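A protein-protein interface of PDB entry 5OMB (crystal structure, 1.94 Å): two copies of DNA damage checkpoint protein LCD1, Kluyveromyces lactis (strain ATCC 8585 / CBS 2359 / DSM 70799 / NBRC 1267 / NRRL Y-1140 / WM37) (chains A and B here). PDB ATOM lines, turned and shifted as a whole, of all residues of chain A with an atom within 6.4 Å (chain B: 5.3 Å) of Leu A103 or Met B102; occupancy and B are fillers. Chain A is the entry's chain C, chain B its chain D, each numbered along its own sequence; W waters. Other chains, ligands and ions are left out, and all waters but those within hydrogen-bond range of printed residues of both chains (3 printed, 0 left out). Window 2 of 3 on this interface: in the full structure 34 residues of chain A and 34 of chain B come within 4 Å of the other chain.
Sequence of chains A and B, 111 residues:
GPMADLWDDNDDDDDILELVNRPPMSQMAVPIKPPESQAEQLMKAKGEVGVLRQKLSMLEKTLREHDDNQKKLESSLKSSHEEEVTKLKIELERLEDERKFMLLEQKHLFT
O of Leu A103 is in hydrogen-bond range of NE2 of Gln A106 (3.4 Å).
Arg B99 touches Glu A98 (NH1 to CG, 3.98 Å). Arg A99 touches Glu B98. CG of Arg A99 touches SD of Met B102, at 3.8 Å. CB of Met B102 touches CE of Met A102, 3.5 Å away. Met A102 touches Leu B103 (CE to CD2, 3.8 Å). CE of Met A102 touches NE2 of Gln B106, at 3.4 Å. CE of Met B102 touches CD2 of Leu A103 (3.9 Å). CB of Lys A107 touches OE1 of Gln B106 (3.7 Å).
Printed residues of chain B within 4 Å of Glu A98: Arg B99. Of the printed residues of chain B, Leu A103 touches Met B102. Leu A104 touches none of the printed residues of chain B. Of the printed residues of chain B, Lys A107 touches Gln B106 (3.7 Å). Of the printed residues of chain A, Glu B98 touches Arg A99 (3.5 Å). Lys B100 touches none of the printed residues of chain A. Of chain A, only Arg A99, Met A102 and Leu A103 come within 4 Å of Met B102. Of the printed residues of chain A, Leu B103 touches Met A102 (3.8 Å). Printed residues of chain A within 4 Å of Gln B106: Met A102 and Lys A107. The nearest residue of chain A that does not touch Met B102 is Glu A98 (6.0 Å).
Hydrophobic or aromatic side chains of chain B within 4 Å of the printed part of chain A: Met B102 and Leu B103.
Arg A99 touches Met B102, but with the chains exchanged Met A102 does not touch Arg B99 (4.1 Å). Met B102 touches its own counterpart, Met A102. Met A102 touches Leu B103, and with the chains exchanged Leu A103 touches Met B102. Met A102 touches Gln B106, but with the chains exchanged Gln A106 does not touch Met B102 (8.8 Å). 9 positions are printed for both chains.
Water W1 lies within hydrogen-bond range of the backbone carbonyl oxygen of Met A102, the backbone NH of Lys A107 and the side-chain amide nitrogen of Gln B106. Water W3 lies within hydrogen-bond range of OE1 of Glu A98 (2.7 Å) and NH1 of Arg B99 (2.8 Å). Water W2 lies within hydrogen-bond range of the side-chain carboxylate of Glu B98 and the guanidinium group of Arg A99.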
ATOM      1  N   GLU A  98      10.245  -4.353  11.988  1.00  0.00           N
ATOM      2  CA  GLU A  98      11.720  -4.281  11.829  1.00  0.00           C
ATOM      3  C   GLU A  98      12.333  -3.376  12.879  1.00  0.00           C
ATOM      4  O   GLU A  98      13.350  -3.733  13.474  1.00  0.00           O
ATOM      5  CB  GLU A  98      12.124  -3.774  10.421  1.00  0.00           C
ATOM      6  CG  GLU A  98      11.882  -4.802   9.332  1.00  0.00           C
ATOM      7  CD  GLU A  98      12.639  -6.094   9.582  1.00  0.00           C
ATOM      8  OE1 GLU A  98      13.874  -6.033   9.762  1.00  0.00           O
ATOM      9  OE2 GLU A  98      11.988  -7.160   9.657  1.00  0.00           O
ATOM     10  N   ARG A  99      11.699  -2.208  13.137  1.00  0.00           N
ATOM     11  CA  ARG A  99      12.182  -1.272  14.161  1.00  0.00           C
ATOM     12  C   ARG A  99      12.117  -1.915  15.554  1.00  0.00           C
ATOM     13  O   ARG A  99      13.088  -1.843  16.304  1.00  0.00           O
ATOM     14  CB  ARG A  99      11.378   0.026  14.128  1.00  0.00           C
ATOM     15  CG  ARG A  99      11.683   0.918  15.334  1.00  0.00           C
ATOM     16  CD  ARG A  99      11.255   2.339  15.115  1.00  0.00           C
ATOM     17  NE  ARG A  99       9.809   2.440  14.980  1.00  0.00           N
ATOM     18  CZ  ARG A  99       9.150   3.586  14.913  1.00  0.00           C
ATOM     19  NH1 ARG A  99       9.800   4.736  14.980  1.00  0.00           N
ATOM     20  NH2 ARG A  99       7.836   3.590  14.794  1.00  0.00           N
ATOM     21  N   LYS A 100      10.992  -2.572  15.884  1.00  0.00           N
ATOM     22  CA  LYS A 100      10.894  -3.262  17.174  1.00  0.00           C
ATOM     23  C   LYS A 100      11.963  -4.393  17.279  1.00  0.00           C
ATOM     24  O   LYS A 100      12.602  -4.506  18.318  1.00  0.00           O
ATOM     25  CB  LYS A 100       9.437  -3.722  17.445  1.00  0.00           C
ATOM     26  CG  LYS A 100       9.227  -5.185  17.769  1.00  0.00           C
ATOM     27  CD  LYS A 100       7.762  -5.582  17.707  1.00  0.00           C
ATOM     28  CE  LYS A 100       7.635  -6.838  16.885  1.00  0.00           C
ATOM     29  NZ  LYS A 100       6.217  -7.248  16.695  1.00  0.00           N
ATOM     30  N   PHE A 101      12.188  -5.185  16.194  1.00  0.00           N
ATOM     31  CA  PHE A 101      13.217  -6.250  16.206  1.00  0.00           C
ATOM     32  C   PHE A 101      14.602  -5.664  16.465  1.00  0.00           C
ATOM     33  O   PHE A 101      15.366  -6.209  17.278  1.00  0.00           O
ATOM     34  CB  PHE A 101      13.214  -7.098  14.913  1.00  0.00           C
ATOM     35  CG  PHE A 101      11.955  -7.887  14.615  1.00  0.00           C
ATOM     36  CD1 PHE A 101      11.137  -8.353  15.649  1.00  0.00           C
ATOM     37  CD2 PHE A 101      11.575  -8.145  13.303  1.00  0.00           C
ATOM     38  CE1 PHE A 101       9.978  -9.071  15.369  1.00  0.00           C
ATOM     39  CE2 PHE A 101      10.389  -8.842  13.019  1.00  0.00           C
ATOM     40  CZ  PHE A 101       9.592  -9.292  14.055  1.00  0.00           C
ATOM     41  N   MET A 102      14.895  -4.507  15.858  1.00  0.00           N
ATOM     42  CA  MET A 102      16.181  -3.829  16.058  1.00  0.00           C
ATOM     43  C   MET A 102      16.385  -3.403  17.498  1.00  0.00           C
ATOM     44  O   MET A 102      17.478  -3.600  18.039  1.00  0.00           O
ATOM     45  CB  MET A 102      16.341  -2.630  15.127  1.00  0.00           C
ATOM     46  CG  MET A 102      16.585  -3.015  13.689  1.00  0.00           C
ATOM     47  SD  MET A 102      16.634  -1.552  12.615  1.00  0.00           S
ATOM     48  CE  MET A 102      18.084  -0.753  13.262  1.00  0.00           C
ATOM     49  N   LEU A 103      15.333  -2.863  18.140  1.00  0.00           N
ATOM     50  CA  LEU A 103      15.434  -2.454  19.545  1.00  0.00           C
ATOM     51  C   LEU A 103      15.585  -3.655  20.464  1.00  0.00           C
ATOM     52  O   LEU A 103      16.376  -3.606  21.400  1.00  0.00           O
ATOM     53  CB  LEU A 103      14.253  -1.576  19.967  1.00  0.00           C
ATOM     54  CG  LEU A 103      14.114  -0.213  19.246  1.00  0.00           C
ATOM     55  CD1 LEU A 103      12.750   0.367  19.472  1.00  0.00           C
ATOM     56  CD2 LEU A 103      15.194   0.786  19.707  1.00  0.00           C
ATOM     57  N   LEU A 104      14.913  -4.769  20.143  1.00  0.00           N
ATOM     58  CA  LEU A 104      15.009  -5.991  20.957  1.00  0.00           C
ATOM     59  C   LEU A 104      16.356  -6.688  20.898  1.00  0.00           C
ATOM     60  O   LEU A 104      16.850  -7.122  21.933  1.00  0.00           O
ATOM     61  CB  LEU A 104      13.917  -6.999  20.536  1.00  0.00           C
ATOM     62  CG  LEU A 104      12.464  -6.679  20.964  1.00  0.00           C
ATOM     63  CD1 LEU A 104      11.484  -7.545  20.182  1.00  0.00           C
ATOM     64  CD2 LEU A 104      12.259  -6.878  22.480  1.00  0.00           C
ATOM     65  N   GLU A 105      16.930  -6.858  19.695  1.00  0.00           N
ATOM     66  CA  GLU A 105      18.151  -7.671  19.505  1.00  0.00           C
ATOM     67  C   GLU A 105      19.453  -6.945  19.888  1.00  0.00           C
ATOM     68  O   GLU A 105      20.493  -7.598  19.915  1.00  0.00           O
ATOM     69  CB  GLU A 105      18.218  -8.266  18.076  1.00  0.00           C
ATOM     70  CG  GLU A 105      18.575  -7.256  17.001  1.00  0.00           C
ATOM     71  CD  GLU A 105      19.060  -7.837  15.687  1.00  0.00           C
ATOM     72  OE1 GLU A 105      19.699  -8.918  15.695  1.00  0.00           O
ATOM     73  OE2 GLU A 105      18.854  -7.169  14.648  1.00  0.00           O
ATOM     74  N   GLN A 106      19.384  -5.627  20.203  1.00  0.00           N
ATOM     75  CA  GLN A 106      20.499  -4.774  20.643  1.00  0.00           C
ATOM     76  C   GLN A 106      21.855  -5.076  19.940  1.00  0.00           C
ATOM     77  O   GLN A 106      22.861  -5.324  20.624  1.00  0.00           O
ATOM     78  CB  GLN A 106      20.631  -4.847  22.178  1.00  0.00           C
ATOM     79  CG  GLN A 106      19.630  -3.952  22.937  1.00  0.00           C
ATOM     80  CD  GLN A 106      18.913  -4.688  24.043  1.00  0.00           C
ATOM     81  OE1 GLN A 106      19.382  -5.704  24.563  1.00  0.00           O
ATOM     82  NE2 GLN A 106      17.749  -4.191  24.434  1.00  0.00           N
ATOM     83  N   LYS A 107      21.867  -5.043  18.569  1.00  0.00           N
ATOM     84  CA  LYS A 107      23.029  -5.332  17.703  1.00  0.00           C
ATOM     85  C   LYS A 107      24.310  -4.552  18.044  1.00  0.00           C
ATOM     86  O   LYS A 107      25.401  -4.997  17.668  1.00  0.00           O
ATOM     87  CB  LYS A 107      22.694  -5.156  16.214  1.00  0.00           C
ATOM     88  CG  LYS A 107      22.549  -6.477  15.473  1.00  0.00           C
ATOM     89  CD  LYS A 107      22.807  -6.370  13.975  1.00  0.00           C
ATOM     90  CE  LYS A 107      22.762  -7.733  13.330  1.00  0.00           C
ATOM     91  NZ  LYS A 107      22.871  -7.651  11.851  1.00  0.00           N
ATOM     92  N   ASP B  97      13.043   6.086   6.759  1.00  0.00           N
ATOM     93  CA  ASP B  97      14.049   7.049   7.248  1.00  0.00           C
ATOM     94  C   ASP B  97      14.474   6.777   8.668  1.00  0.00           C
ATOM     95  O   ASP B  97      15.661   6.821   8.974  1.00  0.00           O
ATOM     96  CB  ASP B  97      13.552   8.494   7.071  1.00  0.00           C
ATOM     97  CG  ASP B  97      13.555   8.958   5.622  1.00  0.00           C
ATOM     98  OD1 ASP B  97      14.175   8.268   4.775  1.00  0.00           O
ATOM     99  OD2 ASP B  97      12.962  10.021   5.340  1.00  0.00           O
ATOM    100  N   GLU B  98      13.508   6.452   9.541  1.00  0.00           N
ATOM    101  CA  GLU B  98      13.765   6.099  10.947  1.00  0.00           C
ATOM    102  C   GLU B  98      14.711   4.881  11.012  1.00  0.00           C
ATOM    103  O   GLU B  98      15.693   4.935  11.729  1.00  0.00           O
ATOM    104  CB  GLU B  98      12.415   5.802  11.634  1.00  0.00           C
ATOM    105  CG  GLU B  98      12.337   6.211  13.082  1.00  0.00           C
ATOM    106  CD  GLU B  98      12.925   7.543  13.506  1.00  0.00           C
ATOM    107  OE1 GLU B  98      12.588   8.585  12.897  1.00  0.00           O
ATOM    108  OE2 GLU B  98      13.711   7.536  14.478  1.00  0.00           O
ATOM    109  N   ARG B  99      14.454   3.813  10.217  1.00  0.00           N
ATOM    110  CA  ARG B  99      15.335   2.634  10.183  1.00  0.00           C
ATOM    111  C   ARG B  99      16.739   2.988   9.637  1.00  0.00           C
ATOM    112  O   ARG B  99      17.747   2.533  10.183  1.00  0.00           O
ATOM    113  CB  ARG B  99      14.693   1.468   9.397  1.00  0.00           C
ATOM    114  CG  ARG B  99      15.747   0.372   9.081  1.00  0.00           C
ATOM    115  CD  ARG B  99      15.186  -0.869   8.438  1.00  0.00           C
ATOM    116  NE  ARG B  99      14.721  -0.602   7.076  1.00  0.00           N
ATOM    117  CZ  ARG B  99      14.183  -1.523   6.291  1.00  0.00           C
ATOM    118  NH1 ARG B  99      14.079  -2.776   6.705  1.00  0.00           N
ATOM    119  NH2 ARG B  99      13.751  -1.199   5.090  1.00  0.00           N
ATOM    120  N   LYS B 100      16.807   3.825   8.590  1.00  0.00           N
ATOM    121  CA  LYS B 100      18.083   4.268   8.003  1.00  0.00           C
ATOM    122  C   LYS B 100      18.899   4.973   9.099  1.00  0.00           C
ATOM    123  O   LYS B 100      20.072   4.652   9.299  1.00  0.00           O
ATOM    124  CB  LYS B 100      17.806   5.202   6.798  1.00  0.00           C
ATOM    125  CG  LYS B 100      18.920   6.197   6.462  1.00  0.00           C
ATOM    126  CD  LYS B 100      18.470   7.208   5.425  1.00  0.00           C
ATOM    127  CE  LYS B 100      17.708   8.404   5.943  1.00  0.00           C
ATOM    128  NZ  LYS B 100      16.934   9.043   4.842  1.00  0.00           N
ATOM    129  N   PHE B 101      18.264   5.899   9.835  1.00  0.00           N
ATOM    130  CA  PHE B 101      18.923   6.607  10.938  1.00  0.00           C
ATOM    131  C   PHE B 101      19.374   5.653  12.053  1.00  0.00           C
ATOM    132  O   PHE B 101      20.485   5.798  12.561  1.00  0.00           O
ATOM    133  CB  PHE B 101      18.015   7.737  11.454  1.00  0.00           C
ATOM    134  CG  PHE B 101      18.013   8.898  10.477  1.00  0.00           C
ATOM    135  CD1 PHE B 101      19.208   9.411   9.974  1.00  0.00           C
ATOM    136  CD2 PHE B 101      16.827   9.512  10.107  1.00  0.00           C
ATOM    137  CE1 PHE B 101      19.208  10.485   9.083  1.00  0.00           C
ATOM    138  CE2 PHE B 101      16.826  10.590   9.220  1.00  0.00           C
ATOM    139  CZ  PHE B 101      18.009  11.054   8.700  1.00  0.00           C
ATOM    140  N   MET B 102      18.545   4.638  12.385  1.00  0.00           N
ATOM    141  CA  MET B 102      18.924   3.646  13.407  1.00  0.00           C
ATOM    142  C   MET B 102      20.142   2.831  12.952  1.00  0.00           C
ATOM    143  O   MET B 102      21.029   2.572  13.766  1.00  0.00           O
ATOM    144  CB  MET B 102      17.762   2.725  13.730  1.00  0.00           C
ATOM    145  CG  MET B 102      16.646   3.380  14.512  1.00  0.00           C
ATOM    146  SD  MET B 102      15.220   2.271  14.658  1.00  0.00           S
ATOM    147  CE  MET B 102      15.817   1.139  15.920  1.00  0.00           C
ATOM    148  N   LEU B 103      20.210   2.468  11.647  1.00  0.00           N
ATOM    149  CA  LEU B 103      21.358   1.748  11.073  1.00  0.00           C
ATOM    150  C   LEU B 103      22.622   2.618  11.040  1.00  0.00           C
ATOM    151  O   LEU B 103      23.725   2.123  11.310  1.00  0.00           O
ATOM    152  CB  LEU B 103      21.048   1.204   9.669  1.00  0.00           C
ATOM    153  CG  LEU B 103      19.983   0.077   9.585  1.00  0.00           C
ATOM    154  CD1 LEU B 103      19.577  -0.182   8.147  1.00  0.00           C
ATOM    155  CD2 LEU B 103      20.458  -1.224  10.291  1.00  0.00           C
ATOM    156  N   LEU B 104      22.468   3.912  10.726  1.00  0.00           N
ATOM    157  CA  LEU B 104      23.595   4.855  10.707  1.00  0.00           C
ATOM    158  C   LEU B 104      24.134   5.064  12.105  1.00  0.00           C
ATOM    159  O   LEU B 104      25.341   5.162  12.275  1.00  0.00           O
ATOM    160  CB  LEU B 104      23.234   6.197  10.038  1.00  0.00           C
ATOM    161  CG  LEU B 104      23.090   6.153   8.503  1.00  0.00           C
ATOM    162  CD1 LEU B 104      22.481   7.392   7.990  1.00  0.00           C
ATOM    163  CD2 LEU B 104      24.440   5.979   7.815  1.00  0.00           C
ATOM    164  N   GLU B 105      23.246   5.038  13.106  1.00  0.00           N
ATOM    165  CA  GLU B 105      23.580   5.123  14.519  1.00  0.00           C
ATOM    166  C   GLU B 105      24.396   3.862  14.876  1.00  0.00           C
ATOM    167  O   GLU B 105      25.440   3.985  15.513  1.00  0.00           O
ATOM    168  CB  GLU B 105      22.295   5.143  15.355  1.00  0.00           C
ATOM    169  CG  GLU B 105      21.998   6.464  16.024  1.00  0.00           C
ATOM    170  CD  GLU B 105      21.194   6.288  17.294  1.00  0.00           C
ATOM    171  OE1 GLU B 105      19.948   6.392  17.228  1.00  0.00           O
ATOM    172  OE2 GLU B 105      21.809   5.991  18.345  1.00  0.00           O
ATOM    173  N   GLN B 106      23.925   2.664  14.439  1.00  0.00           N
ATOM    174  CA  GLN B 106      24.571   1.360  14.676  1.00  0.00           C
ATOM    175  C   GLN B 106      26.019   1.293  14.146  1.00  0.00           C
ATOM    176  O   GLN B 106      26.884   0.740  14.824  1.00  0.00           O
ATOM    177  CB  GLN B 106      23.752   0.234  14.047  1.00  0.00           C
ATOM    178  CG  GLN B 106      22.717  -0.394  14.951  1.00  0.00           C
ATOM    179  CD  GLN B 106      22.211  -1.691  14.355  1.00  0.00           C
ATOM    180  OE1 GLN B 106      22.944  -2.444  13.691  1.00  0.00           O
ATOM    181  NE2 GLN B 106      20.944  -1.986  14.586  1.00  0.00           N
HETATM  182  O   HOH W   1      19.923  -3.743  16.928  1.00  0.00           O
HETATM  183  O   HOH W   2      12.531   5.295  15.901  1.00  0.00           O
HETATM  184  O   HOH W   3      15.525  -4.246   8.605  1.00  0.00           O
